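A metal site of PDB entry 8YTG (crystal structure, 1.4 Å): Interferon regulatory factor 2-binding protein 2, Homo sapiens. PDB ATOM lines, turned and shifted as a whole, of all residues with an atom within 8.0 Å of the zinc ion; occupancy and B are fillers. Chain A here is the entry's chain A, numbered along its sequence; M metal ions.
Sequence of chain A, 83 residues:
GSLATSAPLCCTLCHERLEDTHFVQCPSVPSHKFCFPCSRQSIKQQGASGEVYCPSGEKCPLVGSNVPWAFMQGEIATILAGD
The backbone NH (N) of Glu 58 sits at hydrogen-bond distance from the side-chain hydroxyl (OG) of Ser 56 (3.1 Å).
SG of Cys 60 sits close to OG of Ser 56, 3.8 Å away.
The side-chain hydroxyl (OG) of Ser 56 sits close to a ring nitrogen (ND1) of His 32.
The side-chain sulfur (SG) of Cys 26 sits close to the backbone NH (N) of Val 29 (3.6 Å).
The backbone NH of Trp 69 sits at hydrogen-bond distance from the backbone carbonyl oxygen of Cys 60 (3.0 Å).
The backbone carbonyl oxygen (O) of His 32 sits at hydrogen-bond distance from the side-chain amide nitrogen (NE2) of Gln 25, 3.3 Å away.
The indole nitrogen (NE1) of Trp 69 sits close to the side-chain sulfur (SG) of Cys 26, 3.3 Å away.
The side-chain sulfur (SG) of Cys 54 lies close to the side-chain hydroxyl (OG) of Ser 56, 3.2 Å away.
OG of Ser 56 touches the zinc ion, 3.6 Å away.
Within 4 Å of the zinc ion: Cys 26, His 32, Cys 54, Ser 56 and Cys 60.
The zinc ion is bound by ND1 of His 32 (2.1 Å), SG of Cys 60 (2.3 Å), SG of Cys 26 (2.3 Å) and SG of Cys 54 (2.4 Å).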
ATOM      1  N   THR A  12     -12.237   7.071 -21.918  1.00  0.00           N
ATOM      2  CA  THR A  12     -13.336   7.905 -21.446  1.00  0.00           C
ATOM      3  C   THR A  12     -13.631   7.688 -19.959  1.00  0.00           C
ATOM      4  O   THR A  12     -14.028   8.624 -19.264  1.00  0.00           O
ATOM      5  CB  THR A  12     -14.587   7.580 -22.275  1.00  0.00           C
ATOM      6  OG1 THR A  12     -14.359   7.958 -23.631  1.00  0.00           O
ATOM      7  CG2 THR A  12     -15.831   8.299 -21.760  1.00  0.00           C
ATOM      8  N   GLN A  25     -13.540   1.492 -29.625  1.00  0.00           N
ATOM      9  CA  GLN A  25     -13.995   2.757 -30.191  1.00  0.00           C
ATOM     10  C   GLN A  25     -15.494   2.670 -30.466  1.00  0.00           C
ATOM     11  O   GLN A  25     -15.937   1.858 -31.290  1.00  0.00           O
ATOM     12  CB  GLN A  25     -13.245   3.046 -31.494  1.00  0.00           C
ATOM     13  CG  GLN A  25     -13.751   4.238 -32.229  1.00  0.00           C
ATOM     14  CD  GLN A  25     -13.474   5.487 -31.482  1.00  0.00           C
ATOM     15  OE1 GLN A  25     -12.322   5.889 -31.357  1.00  0.00           O
ATOM     16  NE2 GLN A  25     -14.521   6.137 -30.990  1.00  0.00           N
ATOM     17  N   CYS A  26     -16.271   3.499 -29.770  1.00  0.00           N
ATOM     18  CA  CYS A  26     -17.700   3.572 -30.048  1.00  0.00           C
ATOM     19  C   CYS A  26     -17.908   4.045 -31.485  1.00  0.00           C
ATOM     20  O   CYS A  26     -17.313   5.044 -31.895  1.00  0.00           O
ATOM     21  CB  CYS A  26     -18.301   4.587 -29.078  1.00  0.00           C
ATOM     22  SG  CYS A  26     -20.035   5.032 -29.338  1.00  0.00           S
ATOM     23  N   PRO A  27     -18.745   3.364 -32.269  1.00  0.00           N
ATOM     24  CA  PRO A  27     -18.921   3.751 -33.682  1.00  0.00           C
ATOM     25  C   PRO A  27     -19.524   5.134 -33.890  1.00  0.00           C
ATOM     26  O   PRO A  27     -19.199   5.789 -34.879  1.00  0.00           O
ATOM     27  CB  PRO A  27     -19.841   2.658 -34.223  1.00  0.00           C
ATOM     28  CG  PRO A  27     -19.658   1.492 -33.325  1.00  0.00           C
ATOM     29  CD  PRO A  27     -19.365   2.061 -31.974  1.00  0.00           C
ATOM     30  N   SER A  28     -20.409   5.585 -33.000  1.00  0.00           N
ATOM     31  CA  SER A  28     -21.157   6.816 -33.286  1.00  0.00           C
ATOM     32  C   SER A  28     -20.693   8.013 -32.465  1.00  0.00           C
ATOM     33  O   SER A  28     -21.180   9.123 -32.700  1.00  0.00           O
ATOM     34  CB  SER A  28     -22.649   6.607 -33.058  1.00  0.00           C
ATOM     35  OG  SER A  28     -22.906   6.015 -31.796  1.00  0.00           O
ATOM     36  N   VAL A  29     -19.770   7.812 -31.535  1.00  0.00           N
ATOM     37  CA  VAL A  29     -19.251   8.901 -30.711  1.00  0.00           C
ATOM     38  C   VAL A  29     -17.737   8.745 -30.679  1.00  0.00           C
ATOM     39  O   VAL A  29     -17.212   7.928 -29.904  1.00  0.00           O
ATOM     40  CB  VAL A  29     -19.867   8.881 -29.303  1.00  0.00           C
ATOM     41  CG1 VAL A  29     -19.342  10.076 -28.492  1.00  0.00           C
ATOM     42  CG2 VAL A  29     -21.386   8.895 -29.356  1.00  0.00           C
ATOM     43  N   PRO A  30     -17.002   9.470 -31.520  1.00  0.00           N
ATOM     44  CA  PRO A  30     -15.540   9.295 -31.598  1.00  0.00           C
ATOM     45  C   PRO A  30     -14.829   9.439 -30.265  1.00  0.00           C
ATOM     46  O   PRO A  30     -13.855   8.718 -30.020  1.00  0.00           O
ATOM     47  CB  PRO A  30     -15.122  10.385 -32.587  1.00  0.00           C
ATOM     48  CG  PRO A  30     -16.286  10.552 -33.457  1.00  0.00           C
ATOM     49  CD  PRO A  30     -17.503  10.367 -32.585  1.00  0.00           C
ATOM     50  N   SER A  31     -15.303  10.322 -29.396  1.00  0.00           N
ATOM     51  CA  SER A  31     -14.655  10.537 -28.113  1.00  0.00           C
ATOM     52  C   SER A  31     -14.864   9.390 -27.119  1.00  0.00           C
ATOM     53  O   SER A  31     -14.149   9.341 -26.114  1.00  0.00           O
ATOM     54  CB  SER A  31     -15.089  11.879 -27.508  1.00  0.00           C
ATOM     55  OG  SER A  31     -16.463  11.841 -27.144  1.00  0.00           O
ATOM     56  N   HIS A  32     -15.784   8.469 -27.402  1.00  0.00           N
ATOM     57  CA  HIS A  32     -16.042   7.315 -26.539  1.00  0.00           C
ATOM     58  C   HIS A  32     -15.005   6.240 -26.877  1.00  0.00           C
ATOM     59  O   HIS A  32     -15.178   5.478 -27.821  1.00  0.00           O
ATOM     60  CB  HIS A  32     -17.437   6.771 -26.773  1.00  0.00           C
ATOM     61  CG  HIS A  32     -18.524   7.540 -26.096  1.00  0.00           C
ATOM     62  ND1 HIS A  32     -19.861   7.217 -26.241  1.00  0.00           N
ATOM     63  CD2 HIS A  32     -18.476   8.608 -25.271  1.00  0.00           C
ATOM     64  CE1 HIS A  32     -20.582   8.078 -25.542  1.00  0.00           C
ATOM     65  NE2 HIS A  32     -19.766   8.928 -24.939  1.00  0.00           N
ATOM     66  N   LYS A  33     -13.922   6.193 -26.104  1.00  0.00           N
ATOM     67  CA  LYS A  33     -12.842   5.225 -26.273  1.00  0.00           C
ATOM     68  C   LYS A  33     -12.561   4.591 -24.918  1.00  0.00           C
ATOM     69  O   LYS A  33     -12.528   5.283 -23.901  1.00  0.00           O
ATOM     70  CB  LYS A  33     -11.553   5.841 -26.801  1.00  0.00           C
ATOM     71  CG  LYS A  33     -11.699   6.550 -28.111  1.00  0.00           C
ATOM     72  CD  LYS A  33     -10.541   7.508 -28.331  1.00  0.00           C
ATOM     73  CE  LYS A  33     -10.979   8.674 -29.205  1.00  0.00           C
ATOM     74  NZ  LYS A  33     -10.842   8.304 -30.646  1.00  0.00           N
ATOM     75  N   PHE A  34     -12.351   3.280 -24.896  1.00  0.00           N
ATOM     76  CA  PHE A  34     -12.260   2.556 -23.637  1.00  0.00           C
ATOM     77  C   PHE A  34     -11.096   1.589 -23.647  1.00  0.00           C
ATOM     78  O   PHE A  34     -10.964   0.777 -24.566  1.00  0.00           O
ATOM     79  CB  PHE A  34     -13.561   1.823 -23.357  1.00  0.00           C
ATOM     80  CG  PHE A  34     -14.767   2.697 -23.551  1.00  0.00           C
ATOM     81  CD1 PHE A  34     -15.182   3.548 -22.538  1.00  0.00           C
ATOM     82  CD2 PHE A  34     -15.458   2.692 -24.751  1.00  0.00           C
ATOM     83  CE1 PHE A  34     -16.271   4.362 -22.726  1.00  0.00           C
ATOM     84  CE2 PHE A  34     -16.537   3.502 -24.948  1.00  0.00           C
ATOM     85  CZ  PHE A  34     -16.959   4.343 -23.928  1.00  0.00           C
ATOM     86  N   TYR A  53     -23.628  -2.937 -24.259  1.00  0.00           N
ATOM     87  CA  TYR A  53     -23.734  -1.713 -25.039  1.00  0.00           C
ATOM     88  C   TYR A  53     -22.489  -0.847 -24.801  1.00  0.00           C
ATOM     89  O   TYR A  53     -21.551  -1.241 -24.115  1.00  0.00           O
ATOM     90  CB  TYR A  53     -25.027  -1.001 -24.654  1.00  0.00           C
ATOM     91  CG  TYR A  53     -26.267  -1.854 -24.840  1.00  0.00           C
ATOM     92  CD1 TYR A  53     -26.722  -2.184 -26.103  1.00  0.00           C
ATOM     93  CD2 TYR A  53     -26.948  -2.357 -23.728  1.00  0.00           C
ATOM     94  CE1 TYR A  53     -27.851  -2.973 -26.284  1.00  0.00           C
ATOM     95  CE2 TYR A  53     -28.084  -3.162 -23.910  1.00  0.00           C
ATOM     96  CZ  TYR A  53     -28.527  -3.458 -25.185  1.00  0.00           C
ATOM     97  OH  TYR A  53     -29.639  -4.241 -25.383  1.00  0.00           O
ATOM     98  N   CYS A  54     -22.478   0.360 -25.372  1.00  0.00           N
ATOM     99  CA  CYS A  54     -21.299   1.213 -25.248  1.00  0.00           C
ATOM    100  C   CYS A  54     -20.922   1.373 -23.780  1.00  0.00           C
ATOM    101  O   CYS A  54     -21.782   1.709 -22.956  1.00  0.00           O
ATOM    102  CB  CYS A  54     -21.576   2.607 -25.818  1.00  0.00           C
ATOM    103  SG  CYS A  54     -20.154   3.737 -25.680  1.00  0.00           S
ATOM    104  N   PRO A  55     -19.658   1.172 -23.412  1.00  0.00           N
ATOM    105  CA  PRO A  55     -19.281   1.297 -21.992  1.00  0.00           C
ATOM    106  C   PRO A  55     -19.510   2.685 -21.395  1.00  0.00           C
ATOM    107  O   PRO A  55     -19.422   2.822 -20.169  1.00  0.00           O
ATOM    108  CB  PRO A  55     -17.791   0.944 -21.994  1.00  0.00           C
ATOM    109  CG  PRO A  55     -17.643   0.010 -23.183  1.00  0.00           C
ATOM    110  CD  PRO A  55     -18.564   0.608 -24.233  1.00  0.00           C
ATOM    111  N   SER A  56     -19.803   3.704 -22.202  1.00  0.00           N
ATOM    112  CA  SER A  56     -20.167   5.012 -21.658  1.00  0.00           C
ATOM    113  C   SER A  56     -21.468   4.967 -20.873  1.00  0.00           C
ATOM    114  O   SER A  56     -21.722   5.881 -20.075  1.00  0.00           O
ATOM    115  CB  SER A  56     -20.313   6.026 -22.805  1.00  0.00           C
ATOM    116  OG  SER A  56     -21.447   5.716 -23.595  1.00  0.00           O
ATOM    117  N   GLY A  57     -22.304   3.951 -21.076  1.00  0.00           N
ATOM    118  CA  GLY A  57     -23.639   3.907 -20.524  1.00  0.00           C
ATOM    119  C   GLY A  57     -24.687   4.547 -21.386  1.00  0.00           C
ATOM    120  O   GLY A  57     -25.876   4.418 -21.091  1.00  0.00           O
ATOM    121  N   GLU A  58     -24.296   5.224 -22.463  1.00  0.00           N
ATOM    122  CA  GLU A  58     -25.250   6.031 -23.221  1.00  0.00           C
ATOM    123  C   GLU A  58     -26.002   5.277 -24.307  1.00  0.00           C
ATOM    124  O   GLU A  58     -26.814   5.893 -25.004  1.00  0.00           O
ATOM    125  CB  GLU A  58     -24.553   7.268 -23.786  1.00  0.00           C
ATOM    126  CG  GLU A  58     -24.198   8.258 -22.672  1.00  0.00           C
ATOM    127  CD  GLU A  58     -23.535   9.518 -23.155  1.00  0.00           C
ATOM    128  OE1 GLU A  58     -23.186   9.637 -24.340  1.00  0.00           O
ATOM    129  OE2 GLU A  58     -23.446  10.447 -22.330  1.00  0.00           O
ATOM    130  N   LYS A  59     -25.776   3.964 -24.456  1.00  0.00           N
ATOM    131  CA  LYS A  59     -26.498   3.150 -25.426  1.00  0.00           C
ATOM    132  C   LYS A  59     -26.440   3.760 -26.825  1.00  0.00           C
ATOM    133  O   LYS A  59     -27.422   3.789 -27.560  1.00  0.00           O
ATOM    134  CB  LYS A  59     -27.924   2.836 -24.965  1.00  0.00           C
ATOM    135  CG  LYS A  59     -27.905   2.051 -23.651  1.00  0.00           C
ATOM    136  CD  LYS A  59     -29.256   1.485 -23.257  1.00  0.00           C
ATOM    137  CE  LYS A  59     -29.606   0.276 -24.094  1.00  0.00           C
ATOM    138  NZ  LYS A  59     -31.004  -0.168 -23.847  1.00  0.00           N
ATOM    139  N   CYS A  60     -25.234   4.199 -27.191  1.00  0.00           N
ATOM    140  CA  CYS A  60     -25.009   4.906 -28.437  1.00  0.00           C
ATOM    141  C   CYS A  60     -25.424   4.044 -29.630  1.00  0.00           C
ATOM    142  O   CYS A  60     -25.263   2.825 -29.600  1.00  0.00           O
ATOM    143  CB  CYS A  60     -23.528   5.245 -28.548  1.00  0.00           C
ATOM    144  SG  CYS A  60     -22.933   6.059 -27.039  1.00  0.00           S
ATOM    145  N   PRO A  61     -25.937   4.661 -30.692  1.00  0.00           N
ATOM    146  CA  PRO A  61     -26.445   3.887 -31.826  1.00  0.00           C
ATOM    147  C   PRO A  61     -25.346   3.374 -32.756  1.00  0.00           C
ATOM    148  O   PRO A  61     -24.212   3.852 -32.783  1.00  0.00           O
ATOM    149  CB  PRO A  61     -27.318   4.910 -32.564  1.00  0.00           C
ATOM    150  CG  PRO A  61     -26.656   6.228 -32.268  1.00  0.00           C
ATOM    151  CD  PRO A  61     -26.185   6.106 -30.846  1.00  0.00           C
ATOM    152  N   TRP A  69     -25.587   0.059 -30.610  1.00  0.00           N
ATOM    153  CA  TRP A  69     -24.589  -0.946 -30.973  1.00  0.00           C
ATOM    154  C   TRP A  69     -24.299  -1.815 -29.757  1.00  0.00           C
ATOM    155  O   TRP A  69     -24.487  -1.407 -28.614  1.00  0.00           O
ATOM    156  CB  TRP A  69     -23.322  -0.304 -31.544  1.00  0.00           C
ATOM    157  CG  TRP A  69     -22.388   0.400 -30.556  1.00  0.00           C
ATOM    158  CD1 TRP A  69     -22.400   1.710 -30.220  1.00  0.00           C
ATOM    159  CD2 TRP A  69     -21.297  -0.193 -29.826  1.00  0.00           C
ATOM    160  NE1 TRP A  69     -21.397   1.988 -29.311  1.00  0.00           N
ATOM    161  CE2 TRP A  69     -20.701   0.833 -29.055  1.00  0.00           C
ATOM    162  CE3 TRP A  69     -20.780  -1.491 -29.727  1.00  0.00           C
ATOM    163  CZ2 TRP A  69     -19.611   0.612 -28.209  1.00  0.00           C
ATOM    164  CZ3 TRP A  69     -19.680  -1.715 -28.891  1.00  0.00           C
ATOM    165  CH2 TRP A  69     -19.122  -0.663 -28.138  1.00  0.00           C
HETATM  166 ZN    ZN M   1     -20.680   5.540 -27.153  1.00  0.00          ZN
